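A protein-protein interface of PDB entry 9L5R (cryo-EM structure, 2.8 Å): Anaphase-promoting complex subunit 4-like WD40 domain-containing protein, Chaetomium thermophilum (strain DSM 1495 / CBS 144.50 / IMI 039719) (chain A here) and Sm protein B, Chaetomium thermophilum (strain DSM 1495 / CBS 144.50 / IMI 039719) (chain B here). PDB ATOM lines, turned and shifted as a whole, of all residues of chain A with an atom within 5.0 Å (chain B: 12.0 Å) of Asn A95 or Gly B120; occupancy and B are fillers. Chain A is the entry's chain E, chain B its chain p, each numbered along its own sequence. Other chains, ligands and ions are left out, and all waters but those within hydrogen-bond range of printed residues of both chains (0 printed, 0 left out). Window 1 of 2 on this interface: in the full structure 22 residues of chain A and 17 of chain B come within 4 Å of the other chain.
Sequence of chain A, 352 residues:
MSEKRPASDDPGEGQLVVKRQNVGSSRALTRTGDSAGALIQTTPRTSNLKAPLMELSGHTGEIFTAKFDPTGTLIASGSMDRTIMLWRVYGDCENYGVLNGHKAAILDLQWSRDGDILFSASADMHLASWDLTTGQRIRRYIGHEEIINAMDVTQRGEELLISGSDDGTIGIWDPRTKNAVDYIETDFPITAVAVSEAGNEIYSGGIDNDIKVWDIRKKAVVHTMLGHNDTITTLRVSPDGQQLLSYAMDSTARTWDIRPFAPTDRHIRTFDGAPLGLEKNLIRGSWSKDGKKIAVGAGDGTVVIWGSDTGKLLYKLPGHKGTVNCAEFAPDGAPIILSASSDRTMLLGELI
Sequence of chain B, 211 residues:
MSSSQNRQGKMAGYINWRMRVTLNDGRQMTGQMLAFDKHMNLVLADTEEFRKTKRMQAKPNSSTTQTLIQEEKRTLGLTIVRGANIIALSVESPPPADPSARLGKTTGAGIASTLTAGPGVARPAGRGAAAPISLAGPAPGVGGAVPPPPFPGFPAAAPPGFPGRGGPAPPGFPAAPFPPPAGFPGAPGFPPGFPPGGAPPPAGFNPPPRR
N of Gly B118 is in hydrogen-bond range of O of Asn A95. The backbone NH of Val B121 lies within hydrogen-bond range of the backbone carbonyl oxygen of Ser A57, at 3.1 Å. N of Gly B120 is in hydrogen-bond range of OD1 of Asn A95, at 3.2 Å.
Hydrophobic or aromatic side chains of chain B within 4 Å of the printed part of chain A: Leu B115, Ala B117, Pro B119 and Ala B122. Printed residues of chain A that touch a printed residue of chain B: Ser A57, Met A85, Trp A87, Cys A93, Asn A95, Tyr A96, Gly A97 and Val A98. Hydrophobic or aromatic side chains of chain A within 4 Å of the printed part of chain B: Met A85, Trp A87 and Val A98. Along chain A the printed residues that touch a printed residue of chain B span positions 57 to 98. Among the printed residues, 15 pairs touch across the chains. Among the printed residues, no Asp or Glu carboxylate lies within 4 Å of a Lys or Arg side-chain nitrogen of the other chain.
Among the printed residues, merely in contact across the chains: Ser A57 with Gly B120 (3.2 Å), Met A85 with Gly B120 (3.97 Å), Trp A87 with Gly B120 (3.6 Å), Trp A87 with Val B121 (3.9 Å), Cys A93 with Ala B122 (3.7 Å), Asn A95 with Ala B117 (3.8 Å), Asn A95 with Pro B119 (3.6 Å), Tyr A96 with Leu B115 (3.5 Å), Tyr A96 with Thr B116 (3.8 Å), Gly A97 with Leu B115 (3.7 Å), Val A98 with Gly B118 (3.6 Å) and Val A98 with Pro B119 (3.7 Å).
Of chain B, only Gly B120 (3.2 Å) and Val B121 (3.1 Å) come within 4 Å of Ser A57. No residue of chain B comes within 4 Å of Gly A58. Met A85 touches one residue of chain B. No residue of chain B comes within 4 Å of Leu A86. Cys A93 touches just one residue of chain B: Ala B122 (3.7 Å). No residue of chain B comes within 4 Å of Glu A94. Asn A95 touches just these residues of chain B: Ala B117 (3.8 Å), Gly B118 (3.4 Å), Pro B119 (3.6 Å) and Gly B120 (3.2 Å). Printed residues of chain B within 4 Å of Tyr A96: Leu B115 and Thr B116. Of chain B, only Leu B115 (3.7 Å) comes within 4 Å of Gly A97. Of the printed residues of chain B, Val A98 touches Gly B118 (3.6 Å) and Pro B119 (3.7 Å). Printed residues of chain A within 4 Å of Thr B116: Tyr A96 (3.8 Å). Of the printed residues of chain A, Gly B118 touches Asn A95 (3.4 Å) and Val A98 (3.6 Å). Of the printed residues of chain A, Pro B119 touches Asn A95 and Val A98. Of the printed residues of chain A, Gly B120 touches Ser A57 (3.2 Å), Met A85 (3.97 Å), Trp A87 (3.6 Å) and Asn A95 (3.2 Å). The nearest printed residue of chain A that does not touch Pro B119 is Gly A58 (4.3 Å).
O of Leu A86 is in hydrogen-bond range of N of Tyr A96 (2.7 Å). N of Leu A86 sits at hydrogen-bond distance from O of Gly A97. ND2 of Asn A95 is in hydrogen-bond range of O of Gly A97, 2.9 Å away. The side-chain amide nitrogen (ND2) of Asn A95 is in hydrogen-bond range of the backbone carbonyl oxygen (O) of Leu A86 (2.8 Å).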
ATOM      1  N   SER A  57      13.232  26.302 -13.538  1.00  0.00           N
ATOM      2  CA  SER A  57      13.115  24.857 -13.498  1.00  0.00           C
ATOM      3  C   SER A  57      14.198  24.302 -12.587  1.00  0.00           C
ATOM      4  O   SER A  57      15.217  24.947 -12.341  1.00  0.00           O
ATOM      5  CB  SER A  57      13.233  24.248 -14.899  1.00  0.00           C
ATOM      6  OG  SER A  57      12.734  22.927 -14.923  1.00  0.00           O
ATOM      7  N   GLY A  58      13.976  23.089 -12.097  1.00  0.00           N
ATOM      8  CA  GLY A  58      14.922  22.478 -11.190  1.00  0.00           C
ATOM      9  C   GLY A  58      14.287  21.588 -10.146  1.00  0.00           C
ATOM     10  O   GLY A  58      14.966  20.759  -9.540  1.00  0.00           O
ATOM     11  N   MET A  85      12.786  25.285  -2.823  1.00  0.00           N
ATOM     12  CA  MET A  85      13.818  25.967  -3.589  1.00  0.00           C
ATOM     13  C   MET A  85      13.637  27.471  -3.447  1.00  0.00           C
ATOM     14  O   MET A  85      12.514  27.978  -3.526  1.00  0.00           O
ATOM     15  CB  MET A  85      13.781  25.536  -5.056  1.00  0.00           C
ATOM     16  CG  MET A  85      14.212  24.091  -5.256  1.00  0.00           C
ATOM     17  SD  MET A  85      13.967  23.401  -6.902  1.00  0.00           S
ATOM     18  CE  MET A  85      15.203  24.221  -7.875  1.00  0.00           C
ATOM     19  N   LEU A  86      14.744  28.171  -3.224  1.00  0.00           N
ATOM     20  CA  LEU A  86      14.763  29.588  -2.897  1.00  0.00           C
ATOM     21  C   LEU A  86      15.475  30.335  -4.011  1.00  0.00           C
ATOM     22  O   LEU A  86      16.663  30.084  -4.260  1.00  0.00           O
ATOM     23  CB  LEU A  86      15.482  29.831  -1.569  1.00  0.00           C
ATOM     24  CG  LEU A  86      14.881  29.279  -0.286  1.00  0.00           C
ATOM     25  CD1 LEU A  86      15.843  29.484   0.855  1.00  0.00           C
ATOM     26  CD2 LEU A  86      13.583  29.967  -0.002  1.00  0.00           C
ATOM     27  N   TRP A  87      14.765  31.284  -4.623  1.00  0.00           N
ATOM     28  CA  TRP A  87      15.212  32.037  -5.781  1.00  0.00           C
ATOM     29  C   TRP A  87      15.235  33.531  -5.486  1.00  0.00           C
ATOM     30  O   TRP A  87      14.489  34.029  -4.640  1.00  0.00           O
ATOM     31  CB  TRP A  87      14.296  31.820  -6.986  1.00  0.00           C
ATOM     32  CG  TRP A  87      13.908  30.423  -7.274  1.00  0.00           C
ATOM     33  CD1 TRP A  87      12.942  29.695  -6.655  1.00  0.00           C
ATOM     34  CD2 TRP A  87      14.440  29.592  -8.305  1.00  0.00           C
ATOM     35  NE1 TRP A  87      12.853  28.450  -7.220  1.00  0.00           N
ATOM     36  CE2 TRP A  87      13.764  28.365  -8.239  1.00  0.00           C
ATOM     37  CE3 TRP A  87      15.429  29.767  -9.274  1.00  0.00           C
ATOM     38  CZ2 TRP A  87      14.042  27.319  -9.103  1.00  0.00           C
ATOM     39  CZ3 TRP A  87      15.706  28.725 -10.128  1.00  0.00           C
ATOM     40  CH2 TRP A  87      15.019  27.517 -10.035  1.00  0.00           C
ATOM     41  N   CYS A  93      18.525  35.824 -12.286  1.00  0.00           N
ATOM     42  CA  CYS A  93      17.727  34.994 -11.377  1.00  0.00           C
ATOM     43  C   CYS A  93      18.685  33.950 -10.828  1.00  0.00           C
ATOM     44  O   CYS A  93      19.540  33.452 -11.568  1.00  0.00           O
ATOM     45  CB  CYS A  93      16.493  34.307 -11.987  1.00  0.00           C
ATOM     46  SG  CYS A  93      15.022  35.279 -12.404  1.00  0.00           S
ATOM     47  N   GLU A  94      18.566  33.598  -9.552  1.00  0.00           N
ATOM     48  CA  GLU A  94      19.531  32.703  -8.929  1.00  0.00           C
ATOM     49  C   GLU A  94      18.822  31.807  -7.933  1.00  0.00           C
ATOM     50  O   GLU A  94      18.243  32.301  -6.964  1.00  0.00           O
ATOM     51  CB  GLU A  94      20.640  33.486  -8.219  1.00  0.00           C
ATOM     52  CG  GLU A  94      21.708  34.062  -9.127  1.00  0.00           C
ATOM     53  CD  GLU A  94      22.550  32.994  -9.786  1.00  0.00           C
ATOM     54  OE1 GLU A  94      22.752  31.928  -9.166  1.00  0.00           O
ATOM     55  OE2 GLU A  94      23.014  33.220 -10.923  1.00  0.00           O
ATOM     56  N   ASN A  95      18.887  30.501  -8.154  1.00  0.00           N
ATOM     57  CA  ASN A  95      18.516  29.555  -7.109  1.00  0.00           C
ATOM     58  C   ASN A  95      19.583  29.650  -6.036  1.00  0.00           C
ATOM     59  O   ASN A  95      20.671  29.087  -6.175  1.00  0.00           O
ATOM     60  CB  ASN A  95      18.432  28.135  -7.644  1.00  0.00           C
ATOM     61  CG  ASN A  95      17.849  27.171  -6.635  1.00  0.00           C
ATOM     62  OD1 ASN A  95      17.692  25.983  -6.901  1.00  0.00           O
ATOM     63  ND2 ASN A  95      17.444  27.698  -5.501  1.00  0.00           N
ATOM     64  N   TYR A  96      19.285  30.369  -4.961  1.00  0.00           N
ATOM     65  CA  TYR A  96      20.262  30.545  -3.905  1.00  0.00           C
ATOM     66  C   TYR A  96      20.063  29.596  -2.738  1.00  0.00           C
ATOM     67  O   TYR A  96      20.947  29.515  -1.882  1.00  0.00           O
ATOM     68  CB  TYR A  96      20.259  31.996  -3.405  1.00  0.00           C
ATOM     69  CG  TYR A  96      19.122  32.359  -2.480  1.00  0.00           C
ATOM     70  CD1 TYR A  96      17.881  32.708  -2.984  1.00  0.00           C
ATOM     71  CD2 TYR A  96      19.297  32.383  -1.101  1.00  0.00           C
ATOM     72  CE1 TYR A  96      16.850  33.051  -2.153  1.00  0.00           C
ATOM     73  CE2 TYR A  96      18.267  32.715  -0.264  1.00  0.00           C
ATOM     74  CZ  TYR A  96      17.046  33.049  -0.795  1.00  0.00           C
ATOM     75  OH  TYR A  96      16.012  33.389   0.040  1.00  0.00           O
ATOM     76  N   GLY A  97      18.956  28.871  -2.673  1.00  0.00           N
ATOM     77  CA  GLY A  97      18.741  28.004  -1.525  1.00  0.00           C
ATOM     78  C   GLY A  97      17.981  26.740  -1.851  1.00  0.00           C
ATOM     79  O   GLY A  97      17.132  26.717  -2.742  1.00  0.00           O
ATOM     80  N   VAL A  98      18.295  25.678  -1.114  1.00  0.00           N
ATOM     81  CA  VAL A  98      17.502  24.455  -1.096  1.00  0.00           C
ATOM     82  C   VAL A  98      17.297  24.063   0.359  1.00  0.00           C
ATOM     83  O   VAL A  98      18.261  23.987   1.126  1.00  0.00           O
ATOM     84  CB  VAL A  98      18.172  23.306  -1.876  1.00  0.00           C
ATOM     85  CG1 VAL A  98      17.406  22.010  -1.691  1.00  0.00           C
ATOM     86  CG2 VAL A  98      18.246  23.629  -3.342  1.00  0.00           C
ATOM     87  N   THR B 114      24.264  28.899   5.622  1.00  0.00           N
ATOM     88  CA  THR B 114      24.944  27.800   4.948  1.00  0.00           C
ATOM     89  C   THR B 114      24.093  27.374   3.751  1.00  0.00           C
ATOM     90  O   THR B 114      23.596  26.251   3.690  1.00  0.00           O
ATOM     91  CB  THR B 114      25.173  26.609   5.903  1.00  0.00           C
ATOM     92  OG1 THR B 114      25.583  27.101   7.184  1.00  0.00           O
ATOM     93  CG2 THR B 114      26.276  25.705   5.378  1.00  0.00           C
ATOM     94  N   LEU B 115      23.921  28.290   2.800  1.00  0.00           N
ATOM     95  CA  LEU B 115      23.000  28.097   1.680  1.00  0.00           C
ATOM     96  C   LEU B 115      23.807  27.684   0.457  1.00  0.00           C
ATOM     97  O   LEU B 115      24.332  28.522  -0.276  1.00  0.00           O
ATOM     98  CB  LEU B 115      22.202  29.363   1.385  1.00  0.00           C
ATOM     99  CG  LEU B 115      20.943  29.707   2.183  1.00  0.00           C
ATOM    100  CD1 LEU B 115      19.858  28.661   1.975  1.00  0.00           C
ATOM    101  CD2 LEU B 115      21.229  29.948   3.645  1.00  0.00           C
ATOM    102  N   THR B 116      23.897  26.381   0.229  1.00  0.00           N
ATOM    103  CA  THR B 116      24.497  25.892  -1.002  1.00  0.00           C
ATOM    104  C   THR B 116      23.560  26.182  -2.169  1.00  0.00           C
ATOM    105  O   THR B 116      22.344  25.998  -2.065  1.00  0.00           O
ATOM    106  CB  THR B 116      24.774  24.393  -0.890  1.00  0.00           C
ATOM    107  OG1 THR B 116      25.504  24.138   0.315  1.00  0.00           O
ATOM    108  CG2 THR B 116      25.604  23.907  -2.068  1.00  0.00           C
ATOM    109  N   ALA B 117      24.126  26.672  -3.270  1.00  0.00           N
ATOM    110  CA  ALA B 117      23.324  27.008  -4.439  1.00  0.00           C
ATOM    111  C   ALA B 117      22.724  25.750  -5.050  1.00  0.00           C
ATOM    112  O   ALA B 117      23.383  24.713  -5.150  1.00  0.00           O
ATOM    113  CB  ALA B 117      24.169  27.748  -5.473  1.00  0.00           C
ATOM    114  N   GLY B 118      21.468  25.848  -5.462  1.00  0.00           N
ATOM    115  CA  GLY B 118      20.702  24.682  -5.819  1.00  0.00           C
ATOM    116  C   GLY B 118      20.805  24.258  -7.268  1.00  0.00           C
ATOM    117  O   GLY B 118      21.594  24.793  -8.052  1.00  0.00           O
ATOM    118  N   PRO B 119      19.991  23.271  -7.647  1.00  0.00           N
ATOM    119  CA  PRO B 119      20.035  22.732  -9.009  1.00  0.00           C
ATOM    120  C   PRO B 119      19.426  23.635 -10.063  1.00  0.00           C
ATOM    121  O   PRO B 119      19.560  23.339 -11.254  1.00  0.00           O
ATOM    122  CB  PRO B 119      19.207  21.443  -8.889  1.00  0.00           C
ATOM    123  CG  PRO B 119      19.176  21.127  -7.442  1.00  0.00           C
ATOM    124  CD  PRO B 119      19.168  22.441  -6.757  1.00  0.00           C
ATOM    125  N   GLY B 120      18.752  24.707  -9.661  1.00  0.00           N
ATOM    126  CA  GLY B 120      17.872  25.406 -10.565  1.00  0.00           C
ATOM    127  C   GLY B 120      18.602  26.235 -11.602  1.00  0.00           C
ATOM    128  O   GLY B 120      19.645  26.833 -11.347  1.00  0.00           O
ATOM    129  N   VAL B 121      18.030  26.254 -12.803  1.00  0.00           N
ATOM    130  CA  VAL B 121      18.434  27.168 -13.856  1.00  0.00           C
ATOM    131  C   VAL B 121      17.242  28.058 -14.175  1.00  0.00           C
ATOM    132  O   VAL B 121      16.089  27.720 -13.901  1.00  0.00           O
ATOM    133  CB  VAL B 121      18.938  26.437 -15.119  1.00  0.00           C
ATOM    134  CG1 VAL B 121      19.994  25.409 -14.750  1.00  0.00           C
ATOM    135  CG2 VAL B 121      17.793  25.780 -15.870  1.00  0.00           C
ATOM    136  N   ALA B 122      17.536  29.224 -14.739  1.00  0.00           N
ATOM    137  CA  ALA B 122      16.512  30.179 -15.132  1.00  0.00           C
ATOM    138  C   ALA B 122      16.813  30.677 -16.534  1.00  0.00           C
ATOM    139  O   ALA B 122      17.928  31.129 -16.808  1.00  0.00           O
ATOM    140  CB  ALA B 122      16.442  31.353 -14.159  1.00  0.00           C
ATOM    141  N   ARG B 123      15.823  30.597 -17.413  1.00  0.00           N
ATOM    142  CA  ARG B 123      16.002  30.992 -18.796  1.00  0.00           C
ATOM    143  C   ARG B 123      14.790  31.778 -19.268  1.00  0.00           C
ATOM    144  O   ARG B 123      13.680  31.574 -18.763  1.00  0.00           O
ATOM    145  CB  ARG B 123      16.210  29.769 -19.700  1.00  0.00           C
ATOM    146  CG  ARG B 123      15.060  28.792 -19.689  1.00  0.00           C
ATOM    147  CD  ARG B 123      15.267  27.704 -20.712  1.00  0.00           C
ATOM    148  NE  ARG B 123      14.051  26.937 -20.956  1.00  0.00           N
ATOM    149  CZ  ARG B 123      13.095  27.300 -21.800  1.00  0.00           C
ATOM    150  NH1 ARG B 123      13.164  28.434 -22.476  1.00  0.00           N
ATOM    151  NH2 ARG B 123      12.051  26.498 -21.980  1.00  0.00           N
ATOM    152  N   PRO B 124      14.978  32.701 -20.205  1.00  0.00           N
ATOM    153  CA  PRO B 124      13.829  33.318 -20.868  1.00  0.00           C
ATOM    154  C   PRO B 124      13.061  32.299 -21.691  1.00  0.00           C
ATOM    155  O   PRO B 124      13.630  31.365 -22.256  1.00  0.00           O
ATOM    156  CB  PRO B 124      14.464  34.385 -21.765  1.00  0.00           C
ATOM    157  CG  PRO B 124      15.783  34.654 -21.154  1.00  0.00           C
ATOM    158  CD  PRO B 124      16.241  33.362 -20.565  1.00  0.00           C
